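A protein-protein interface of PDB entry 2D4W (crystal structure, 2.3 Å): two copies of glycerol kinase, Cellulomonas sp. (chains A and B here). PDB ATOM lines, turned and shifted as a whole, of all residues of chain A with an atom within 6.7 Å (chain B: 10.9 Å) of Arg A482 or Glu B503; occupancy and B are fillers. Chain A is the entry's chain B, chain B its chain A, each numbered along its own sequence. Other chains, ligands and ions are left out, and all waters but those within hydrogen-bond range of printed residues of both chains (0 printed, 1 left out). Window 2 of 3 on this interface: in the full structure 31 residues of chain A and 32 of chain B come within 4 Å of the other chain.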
ATOM      1  N   ASN A 340     -19.197  17.906 -20.151  1.00  0.00           N
ATOM      2  CA  ASN A 340     -18.319  17.906 -21.293  1.00  0.00           C
ATOM      3  C   ASN A 340     -16.877  17.581 -20.937  1.00  0.00           C
ATOM      4  O   ASN A 340     -16.009  17.530 -21.810  1.00  0.00           O
ATOM      5  CB  ASN A 340     -18.420  19.226 -22.028  1.00  0.00           C
ATOM      6  CG  ASN A 340     -18.027  20.414 -21.174  1.00  0.00           C
ATOM      7  OD1 ASN A 340     -17.067  20.362 -20.396  1.00  0.00           O
ATOM      8  ND2 ASN A 340     -18.733  21.497 -21.350  1.00  0.00           N
ATOM      9  N   GLY A 341     -16.618  17.386 -19.649  1.00  0.00           N
ATOM     10  CA  GLY A 341     -15.287  17.005 -19.204  1.00  0.00           C
ATOM     11  C   GLY A 341     -14.243  18.113 -19.414  1.00  0.00           C
ATOM     12  O   GLY A 341     -13.052  17.879 -19.267  1.00  0.00           O
ATOM     13  N   GLY A 342     -14.680  19.331 -19.688  1.00  0.00           N
ATOM     14  CA  GLY A 342     -13.726  20.380 -19.943  1.00  0.00           C
ATOM     15  C   GLY A 342     -13.644  20.680 -21.445  1.00  0.00           C
ATOM     16  O   GLY A 342     -13.017  21.653 -21.831  1.00  0.00           O
ATOM     17  N   ALA A 343     -14.223  19.839 -22.300  1.00  0.00           N
ATOM     18  CA  ALA A 343     -14.115  20.074 -23.745  1.00  0.00           C
ATOM     19  C   ALA A 343     -15.200  20.963 -24.366  1.00  0.00           C
ATOM     20  O   ALA A 343     -16.375  20.915 -23.935  1.00  0.00           O
ATOM     21  CB  ALA A 343     -14.050  18.780 -24.483  1.00  0.00           C
ATOM     22  N   TYR A 344     -14.788  21.760 -25.357  1.00  0.00           N
ATOM     23  CA  TYR A 344     -15.651  22.657 -26.099  1.00  0.00           C
ATOM     24  C   TYR A 344     -15.320  22.627 -27.591  1.00  0.00           C
ATOM     25  O   TYR A 344     -14.148  22.701 -27.999  1.00  0.00           O
ATOM     26  CB  TYR A 344     -15.513  24.111 -25.607  1.00  0.00           C
ATOM     27  CG  TYR A 344     -15.868  24.293 -24.133  1.00  0.00           C
ATOM     28  CD1 TYR A 344     -17.113  24.762 -23.763  1.00  0.00           C
ATOM     29  CD2 TYR A 344     -14.946  23.995 -23.134  1.00  0.00           C
ATOM     30  CE1 TYR A 344     -17.441  24.917 -22.440  1.00  0.00           C
ATOM     31  CE2 TYR A 344     -15.272  24.155 -21.790  1.00  0.00           C
ATOM     32  CZ  TYR A 344     -16.521  24.605 -21.458  1.00  0.00           C
ATOM     33  OH  TYR A 344     -16.867  24.746 -20.143  1.00  0.00           O
ATOM     34  N   GLY A 367      -9.919  22.360 -24.793  1.00  0.00           N
ATOM     35  CA  GLY A 367     -10.077  21.858 -23.437  1.00  0.00           C
ATOM     36  C   GLY A 367      -9.885  20.354 -23.351  1.00  0.00           C
ATOM     37  O   GLY A 367     -10.541  19.672 -22.535  1.00  0.00           O
ATOM     38  N   GLN A 426     -29.767  26.179 -21.268  1.00  0.00           N
ATOM     39  CA  GLN A 426     -29.019  27.340 -21.778  1.00  0.00           C
ATOM     40  C   GLN A 426     -29.864  28.580 -22.089  1.00  0.00           C
ATOM     41  O   GLN A 426     -29.393  29.722 -21.946  1.00  0.00           O
ATOM     42  CB  GLN A 426     -28.190  26.939 -23.011  1.00  0.00           C
ATOM     43  CG  GLN A 426     -26.941  26.154 -22.631  1.00  0.00           C
ATOM     44  CD  GLN A 426     -25.974  27.054 -21.897  1.00  0.00           C
ATOM     45  OE1 GLN A 426     -25.897  28.187 -22.213  1.00  0.00           O
ATOM     46  NE2 GLN A 426     -25.263  26.545 -20.933  1.00  0.00           N
ATOM     47  N   SER A 477     -27.834  28.564 -12.390  1.00  0.00           N
ATOM     48  CA  SER A 477     -27.319  29.727 -13.102  1.00  0.00           C
ATOM     49  C   SER A 477     -25.811  29.792 -13.242  1.00  0.00           C
ATOM     50  O   SER A 477     -25.285  30.327 -14.229  1.00  0.00           O
ATOM     51  CB  SER A 477     -27.776  30.980 -12.392  1.00  0.00           C
ATOM     52  OG  SER A 477     -29.147  31.158 -12.635  1.00  0.00           O
ATOM     53  N   GLY A 478     -25.109  29.277 -12.248  1.00  0.00           N
ATOM     54  CA  GLY A 478     -23.662  29.330 -12.289  1.00  0.00           C
ATOM     55  C   GLY A 478     -23.090  28.409 -13.345  1.00  0.00           C
ATOM     56  O   GLY A 478     -22.207  28.789 -14.129  1.00  0.00           O
ATOM     57  N   GLU A 479     -23.594  27.184 -13.363  1.00  0.00           N
ATOM     58  CA  GLU A 479     -23.098  26.198 -14.304  1.00  0.00           C
ATOM     59  C   GLU A 479     -23.459  26.648 -15.707  1.00  0.00           C
ATOM     60  O   GLU A 479     -22.633  26.596 -16.603  1.00  0.00           O
ATOM     61  CB  GLU A 479     -23.627  24.796 -13.981  1.00  0.00           C
ATOM     62  CG  GLU A 479     -23.310  23.742 -15.026  1.00  0.00           C
ATOM     63  CD  GLU A 479     -21.844  23.287 -15.045  1.00  0.00           C
ATOM     64  OE1 GLU A 479     -21.544  22.367 -15.838  1.00  0.00           O
ATOM     65  OE2 GLU A 479     -20.994  23.823 -14.282  1.00  0.00           O
ATOM     66  N   ARG A 480     -24.677  27.146 -15.850  1.00  0.00           N
ATOM     67  CA  ARG A 480     -25.226  27.614 -17.105  1.00  0.00           C
ATOM     68  C   ARG A 480     -24.343  28.659 -17.753  1.00  0.00           C
ATOM     69  O   ARG A 480     -23.975  28.563 -18.924  1.00  0.00           O
ATOM     70  CB  ARG A 480     -26.611  28.233 -16.850  1.00  0.00           C
ATOM     71  CG  ARG A 480     -27.209  29.033 -18.033  1.00  0.00           C
ATOM     72  CD  ARG A 480     -28.516  29.813 -17.710  1.00  0.00           C
ATOM     73  NE  ARG A 480     -29.152  30.351 -18.911  1.00  0.00           N
ATOM     74  CZ  ARG A 480     -29.873  31.480 -18.969  1.00  0.00           C
ATOM     75  NH1 ARG A 480     -30.094  32.207 -17.876  1.00  0.00           N
ATOM     76  NH2 ARG A 480     -30.397  31.888 -20.125  1.00  0.00           N
ATOM     77  N   GLU A 481     -24.011  29.674 -16.983  1.00  0.00           N
ATOM     78  CA  GLU A 481     -23.238  30.768 -17.518  1.00  0.00           C
ATOM     79  C   GLU A 481     -21.783  30.408 -17.668  1.00  0.00           C
ATOM     80  O   GLU A 481     -21.138  30.830 -18.605  1.00  0.00           O
ATOM     81  CB  GLU A 481     -23.412  32.012 -16.646  1.00  0.00           C
ATOM     82  CG  GLU A 481     -24.847  32.550 -16.693  1.00  0.00           C
ATOM     83  CD  GLU A 481     -25.268  32.955 -18.109  1.00  0.00           C
ATOM     84  OE1 GLU A 481     -26.476  33.043 -18.397  1.00  0.00           O
ATOM     85  OE2 GLU A 481     -24.382  33.244 -18.932  1.00  0.00           O
ATOM     86  N   ARG A 482     -21.257  29.618 -16.764  1.00  0.00           N
ATOM     87  CA  ARG A 482     -19.862  29.248 -16.870  1.00  0.00           C
ATOM     88  C   ARG A 482     -19.582  28.485 -18.178  1.00  0.00           C
ATOM     89  O   ARG A 482     -18.604  28.779 -18.889  1.00  0.00           O
ATOM     90  CB  ARG A 482     -19.484  28.370 -15.710  1.00  0.00           C
ATOM     91  CG  ARG A 482     -18.051  28.463 -15.379  1.00  0.00           C
ATOM     92  CD  ARG A 482     -17.600  27.419 -14.430  1.00  0.00           C
ATOM     93  NE  ARG A 482     -17.187  26.267 -15.187  1.00  0.00           N
ATOM     94  CZ  ARG A 482     -17.870  25.148 -15.271  1.00  0.00           C
ATOM     95  NH1 ARG A 482     -19.017  25.065 -14.628  1.00  0.00           N
ATOM     96  NH2 ARG A 482     -17.408  24.120 -15.994  1.00  0.00           N
ATOM     97  N   LEU A 483     -20.409  27.483 -18.453  1.00  0.00           N
ATOM     98  CA  LEU A 483     -20.300  26.743 -19.715  1.00  0.00           C
ATOM     99  C   LEU A 483     -20.371  27.663 -20.930  1.00  0.00           C
ATOM    100  O   LEU A 483     -19.511  27.622 -21.791  1.00  0.00           O
ATOM    101  CB  LEU A 483     -21.401  25.712 -19.830  1.00  0.00           C
ATOM    102  CG  LEU A 483     -21.293  24.526 -18.890  1.00  0.00           C
ATOM    103  CD1 LEU A 483     -22.574  23.816 -18.924  1.00  0.00           C
ATOM    104  CD2 LEU A 483     -20.139  23.599 -19.281  1.00  0.00           C
ATOM    105  N   TYR A 484     -21.358  28.546 -20.956  1.00  0.00           N
ATOM    106  CA  TYR A 484     -21.547  29.448 -22.092  1.00  0.00           C
ATOM    107  C   TYR A 484     -20.426  30.458 -22.324  1.00  0.00           C
ATOM    108  O   TYR A 484     -20.029  30.703 -23.468  1.00  0.00           O
ATOM    109  CB  TYR A 484     -22.867  30.193 -21.957  1.00  0.00           C
ATOM    110  CG  TYR A 484     -23.302  31.001 -23.168  1.00  0.00           C
ATOM    111  CD1 TYR A 484     -23.323  30.439 -24.448  1.00  0.00           C
ATOM    112  CD2 TYR A 484     -23.726  32.320 -23.035  1.00  0.00           C
ATOM    113  CE1 TYR A 484     -23.759  31.176 -25.575  1.00  0.00           C
ATOM    114  CE2 TYR A 484     -24.159  33.048 -24.138  1.00  0.00           C
ATOM    115  CZ  TYR A 484     -24.185  32.468 -25.403  1.00  0.00           C
ATOM    116  OH  TYR A 484     -24.601  33.235 -26.509  1.00  0.00           O
ATOM    117  N   ARG A 485     -19.932  31.085 -21.263  1.00  0.00           N
ATOM    118  CA  ARG A 485     -18.861  32.056 -21.464  1.00  0.00           C
ATOM    119  C   ARG A 485     -17.518  31.398 -21.769  1.00  0.00           C
ATOM    120  O   ARG A 485     -16.657  32.002 -22.401  1.00  0.00           O
ATOM    121  CB  ARG A 485     -18.747  33.079 -20.305  1.00  0.00           C
ATOM    122  CG  ARG A 485     -18.072  32.570 -19.044  1.00  0.00           C
ATOM    123  CD  ARG A 485     -18.029  33.638 -17.855  1.00  0.00           C
ATOM    124  NE  ARG A 485     -19.288  34.399 -17.765  1.00  0.00           N
ATOM    125  CZ  ARG A 485     -20.032  34.530 -16.663  1.00  0.00           C
ATOM    126  NH1 ARG A 485     -19.647  33.969 -15.529  1.00  0.00           N
ATOM    127  NH2 ARG A 485     -21.171  35.219 -16.700  1.00  0.00           N
ATOM    128  N   ASN A 486     -17.344  30.185 -21.272  1.00  0.00           N
ATOM    129  CA  ASN A 486     -16.159  29.419 -21.565  1.00  0.00           C
ATOM    130  C   ASN A 486     -16.179  29.118 -23.084  1.00  0.00           C
ATOM    131  O   ASN A 486     -15.165  29.268 -23.803  1.00  0.00           O
ATOM    132  CB  ASN A 486     -16.185  28.111 -20.818  1.00  0.00           C
ATOM    133  CG  ASN A 486     -15.464  28.147 -19.441  1.00  0.00           C
ATOM    134  OD1 ASN A 486     -14.668  29.032 -19.128  1.00  0.00           O
ATOM    135  ND2 ASN A 486     -15.744  27.138 -18.633  1.00  0.00           N
ATOM    136  N   TRP A 487     -17.347  28.740 -23.584  1.00  0.00           N
ATOM    137  CA  TRP A 487     -17.472  28.397 -24.981  1.00  0.00           C
ATOM    138  C   TRP A 487     -17.266  29.632 -25.833  1.00  0.00           C
ATOM    139  O   TRP A 487     -16.603  29.577 -26.874  1.00  0.00           O
ATOM    140  CB  TRP A 487     -18.858  27.782 -25.248  1.00  0.00           C
ATOM    141  CG  TRP A 487     -19.122  27.487 -26.633  1.00  0.00           C
ATOM    142  CD1 TRP A 487     -18.726  26.378 -27.329  1.00  0.00           C
ATOM    143  CD2 TRP A 487     -19.837  28.305 -27.559  1.00  0.00           C
ATOM    144  NE1 TRP A 487     -19.189  26.441 -28.619  1.00  0.00           N
ATOM    145  CE2 TRP A 487     -19.885  27.606 -28.789  1.00  0.00           C
ATOM    146  CE3 TRP A 487     -20.495  29.543 -27.459  1.00  0.00           C
ATOM    147  CZ2 TRP A 487     -20.523  28.121 -29.930  1.00  0.00           C
ATOM    148  CZ3 TRP A 487     -21.133  30.048 -28.547  1.00  0.00           C
ATOM    149  CH2 TRP A 487     -21.145  29.332 -29.796  1.00  0.00           C
ATOM    150  N   ASP B 360       0.517  23.622 -19.428  1.00  0.00           N
ATOM    151  CA  ASP B 360      -0.809  23.288 -18.903  1.00  0.00           C
ATOM    152  C   ASP B 360      -1.270  21.916 -19.440  1.00  0.00           C
ATOM    153  O   ASP B 360      -0.769  21.421 -20.459  1.00  0.00           O
ATOM    154  CB  ASP B 360      -1.816  24.378 -19.301  1.00  0.00           C
ATOM    155  CG  ASP B 360      -3.157  24.263 -18.562  1.00  0.00           C
ATOM    156  OD1 ASP B 360      -3.371  25.031 -17.600  1.00  0.00           O
ATOM    157  OD2 ASP B 360      -4.082  23.475 -18.900  1.00  0.00           O
ATOM    158  N   ALA B 361      -2.193  21.303 -18.699  1.00  0.00           N
ATOM    159  CA  ALA B 361      -2.724  19.972 -18.999  1.00  0.00           C
ATOM    160  C   ALA B 361      -3.794  20.019 -20.086  1.00  0.00           C
ATOM    161  O   ALA B 361      -4.216  19.000 -20.595  1.00  0.00           O
ATOM    162  CB  ALA B 361      -3.321  19.324 -17.725  1.00  0.00           C
ATOM    163  N   ARG B 362      -4.219  21.221 -20.432  1.00  0.00           N
ATOM    164  CA  ARG B 362      -5.240  21.403 -21.446  1.00  0.00           C
ATOM    165  C   ARG B 362      -4.611  21.680 -22.816  1.00  0.00           C
ATOM    166  O   ARG B 362      -3.785  22.588 -22.958  1.00  0.00           O
ATOM    167  CB  ARG B 362      -6.173  22.544 -21.068  1.00  0.00           C
ATOM    168  CG  ARG B 362      -7.245  22.160 -20.025  1.00  0.00           C
ATOM    169  CD  ARG B 362      -7.860  23.371 -19.311  1.00  0.00           C
ATOM    170  NE  ARG B 362      -6.904  23.976 -18.370  1.00  0.00           N
ATOM    171  CZ  ARG B 362      -7.162  25.056 -17.613  1.00  0.00           C
ATOM    172  NH1 ARG B 362      -8.358  25.651 -17.677  1.00  0.00           N
ATOM    173  NH2 ARG B 362      -6.247  25.543 -16.788  1.00  0.00           N
ATOM    174  N   GLY B 363      -5.045  20.892 -23.797  1.00  0.00           N
ATOM    175  CA  GLY B 363      -4.598  20.969 -25.170  1.00  0.00           C
ATOM    176  C   GLY B 363      -5.786  21.265 -26.086  1.00  0.00           C
ATOM    177  O   GLY B 363      -6.922  21.460 -25.618  1.00  0.00           O
ATOM    178  N   TRP B 497      -6.669  30.941 -24.154  1.00  0.00           N
ATOM    179  CA  TRP B 497      -8.008  30.445 -23.806  1.00  0.00           C
ATOM    180  C   TRP B 497      -8.000  29.748 -22.456  1.00  0.00           C
ATOM    181  O   TRP B 497      -8.871  29.934 -21.633  1.00  0.00           O
ATOM    182  CB  TRP B 497      -8.576  29.438 -24.840  1.00  0.00           C
ATOM    183  CG  TRP B 497      -9.885  28.920 -24.360  1.00  0.00           C
ATOM    184  CD1 TRP B 497     -11.066  29.611 -24.342  1.00  0.00           C
ATOM    185  CD2 TRP B 497     -10.164  27.640 -23.757  1.00  0.00           C
ATOM    186  NE1 TRP B 497     -12.043  28.845 -23.757  1.00  0.00           N
ATOM    187  CE2 TRP B 497     -11.521  27.634 -23.391  1.00  0.00           C
ATOM    188  CE3 TRP B 497      -9.413  26.490 -23.509  1.00  0.00           C
ATOM    189  CZ2 TRP B 497     -12.161  26.512 -22.845  1.00  0.00           C
ATOM    190  CZ3 TRP B 497     -10.030  25.392 -22.876  1.00  0.00           C
ATOM    191  CH2 TRP B 497     -11.396  25.410 -22.583  1.00  0.00           C
ATOM    192  N   VAL B 498      -6.994  28.937 -22.274  1.00  0.00           N
ATOM    193  CA  VAL B 498      -6.778  28.200 -21.057  1.00  0.00           C
ATOM    194  C   VAL B 498      -6.695  29.114 -19.799  1.00  0.00           C
ATOM    195  O   VAL B 498      -7.229  28.755 -18.736  1.00  0.00           O
ATOM    196  CB  VAL B 498      -5.501  27.294 -21.240  1.00  0.00           C
ATOM    197  CG1 VAL B 498      -4.902  26.899 -19.946  1.00  0.00           C
ATOM    198  CG2 VAL B 498      -5.858  26.077 -22.097  1.00  0.00           C
ATOM    199  N   ASP B 499      -6.049  30.276 -19.918  1.00  0.00           N
ATOM    200  CA  ASP B 499      -5.973  31.193 -18.781  1.00  0.00           C
ATOM    201  C   ASP B 499      -7.372  31.701 -18.449  1.00  0.00           C
ATOM    202  O   ASP B 499      -7.742  31.821 -17.315  1.00  0.00           O
ATOM    203  CB  ASP B 499      -5.070  32.385 -19.087  1.00  0.00           C
ATOM    204  CG  ASP B 499      -3.614  31.982 -19.259  1.00  0.00           C
ATOM    205  OD1 ASP B 499      -3.184  30.952 -18.664  1.00  0.00           O
ATOM    206  OD2 ASP B 499      -2.833  32.649 -19.974  1.00  0.00           O
ATOM    207  N   GLU B 500      -8.168  31.993 -19.457  1.00  0.00           N
ATOM    208  CA  GLU B 500      -9.489  32.496 -19.168  1.00  0.00           C
ATOM    209  C   GLU B 500     -10.493  31.372 -19.006  1.00  0.00           C
ATOM    210  O   GLU B 500     -11.672  31.628 -18.887  1.00  0.00           O
ATOM    211  CB  GLU B 500      -9.951  33.499 -20.234  1.00  0.00           C
ATOM    212  CG  GLU B 500      -9.872  33.047 -21.678  1.00  0.00           C
ATOM    213  CD  GLU B 500     -10.422  34.075 -22.665  1.00  0.00           C
ATOM    214  OE1 GLU B 500     -10.434  33.801 -23.876  1.00  0.00           O
ATOM    215  OE2 GLU B 500     -10.869  35.176 -22.269  1.00  0.00           O
ATOM    216  N   ASP B 501     -10.046  30.123 -18.967  1.00  0.00           N
ATOM    217  CA  ASP B 501     -10.980  28.992 -18.903  1.00  0.00           C
ATOM    218  C   ASP B 501     -11.436  28.614 -17.492  1.00  0.00           C
ATOM    219  O   ASP B 501     -10.697  28.012 -16.732  1.00  0.00           O
ATOM    220  CB  ASP B 501     -10.368  27.788 -19.616  1.00  0.00           C
ATOM    221  CG  ASP B 501     -11.198  26.518 -19.462  1.00  0.00           C
ATOM    222  OD1 ASP B 501     -12.442  26.555 -19.584  1.00  0.00           O
ATOM    223  OD2 ASP B 501     -10.658  25.417 -19.266  1.00  0.00           O
ATOM    224  N   VAL B 502     -12.681  28.893 -17.161  1.00  0.00           N
ATOM    225  CA  VAL B 502     -13.128  28.709 -15.782  1.00  0.00           C
ATOM    226  C   VAL B 502     -13.690  27.300 -15.583  1.00  0.00           C
ATOM    227  O   VAL B 502     -14.760  26.981 -16.073  1.00  0.00           O
ATOM    228  CB  VAL B 502     -14.103  29.875 -15.400  1.00  0.00           C
ATOM    229  CG1 VAL B 502     -14.776  29.682 -14.044  1.00  0.00           C
ATOM    230  CG2 VAL B 502     -13.359  31.193 -15.457  1.00  0.00           C
ATOM    231  N   GLU B 503     -12.936  26.427 -14.928  1.00  0.00           N
ATOM    232  CA  GLU B 503     -13.400  25.066 -14.787  1.00  0.00           C
ATOM    233  C   GLU B 503     -14.040  24.855 -13.400  1.00  0.00           C
ATOM    234  O   GLU B 503     -14.895  25.668 -12.987  1.00  0.00           O
ATOM    235  CB  GLU B 503     -12.268  24.048 -15.075  1.00  0.00           C
ATOM    236  CG  GLU B 503     -11.991  23.795 -16.575  1.00  0.00           C
ATOM    237  CD  GLU B 503     -13.267  23.571 -17.407  1.00  0.00           C
ATOM    238  OE1 GLU B 503     -14.050  22.667 -17.068  1.00  0.00           O
ATOM    239  OE2 GLU B 503     -13.516  24.289 -18.403  1.00  0.00           O
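Gly A342 touches Glu B503 (CA to OE1, 3.7 Å). CD2 of Tyr A344 touches CZ2 of Trp B497, at 3.8 Å. OH of Tyr A344 touches OE2 of Glu B503, at 3.8 Å. CA of Gly A367 touches CZ3 of Trp B497, at 3.6 Å. Glu B500 touches Asn A486 (O to OD1, 3.97 Å). ND2 of Asn A486 touches OE2 of Glu B503, at 3.6 Å.
The backbone NH (N) of Gly A367 is in hydrogen-bond range of the backbone carbonyl oxygen (O) of Gly B363 (3.2 Å). The indole nitrogen (NE1) of Trp B497 is in hydrogen-bond range of the backbone carbonyl oxygen (O) of Asn A486 (3.2 Å). The side-chain carboxylate (OD1) of Asp B501 sits close to the side-chain amide oxygen (OD1) of Asn A486. The backbone carbonyl oxygen (O) of Val B502 sits at hydrogen-bond distance from the guanidinium group (NE) of Arg A482, at 2.7 Å. The backbone carbonyl oxygen (O) of Val B502 sits at hydrogen-bond distance from the side-chain amide nitrogen (ND2) of Asn A486, 2.7 Å away. The guanidinium group (NH2) of Arg A482 is in salt-bridge range of the side-chain carboxylate (OE1) of Glu B503 (3.8 Å).
No position is printed for both chains.
Hydrophobic or aromatic side chains of chain A within 4 Å of the printed part of chain B: Tyr A344. Of the 11 printed residues of chain B, 6 touch a printed residue of chain A. Along chain B the printed residues that touch a printed residue of chain A span positions 363 to 503. Among the printed residues, 12 pairs touch across the chains. Among the printed residues, Asp or Glu carboxylates within 4 Å of a Lys or Arg side-chain nitrogen of the other chain: Arg A482 with Glu B503.
The guanidinium group (NH1) of Arg B362 is in salt-bridge range of the side-chain carboxylate (OD2) of Asp B501 (2.8 Å). OD1 of Asn A340 is in hydrogen-bond range of N of Gly A342, at 2.7 Å. The side-chain amide nitrogen (ND2) of Asn A486 lies within hydrogen-bond range of the side-chain hydroxyl (OH) of Tyr A344 (3.0 Å). OE1 of Glu A479 lies within salt-bridge range of NH1 of Arg A482. O of Arg A482 sits close to ND2 of Asn A486 (3.3 Å).
No residue of chain B comes within 4 Å of Gly A341. Gly A342 touches just one residue of chain B: Glu B503 (3.7 Å). Printed residues of chain B within 4 Å of Tyr A344: Trp B497 and Glu B503. Printed residues of chain B within 4 Å of Gly A367: Gly B363 and Trp B497. Glu A479 touches none of the printed residues of chain B. No residue of chain B comes within 4 Å of Glu A481. Of chain B, only Val B502 (2.7 Å) and Glu B503 (3.2 Å) come within 4 Å of Arg A482. No residue of chain B comes within 4 Å of Leu A483. Arg A485 touches none of the printed residues of chain B. Of chain B, only Trp B497 (3.2 Å), Glu B500 (3.97 Å), Asp B501 (3.4 Å), Val B502 (2.7 Å) and Glu B503 (3.6 Å) come within 4 Å of Asn A486. Printed residues of chain A within 4 Å of Trp B497: Tyr A344, Gly A367 and Asn A486. Asp B499 touches none of the printed residues of chain A. Glu B503 touches just these residues of chain A: Gly A342, Tyr A344, Arg A482 and Asn A486. The nearest residue of chain B that does not touch Arg A482 is Asp B501 (6.5 Å). The nearest residue of chain A that does not touch Glu B503 is Asn A340 (5.0 Å). The nearest printed residue of chain B that does not touch Tyr A344 is Asp B501 (4.3 Å).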
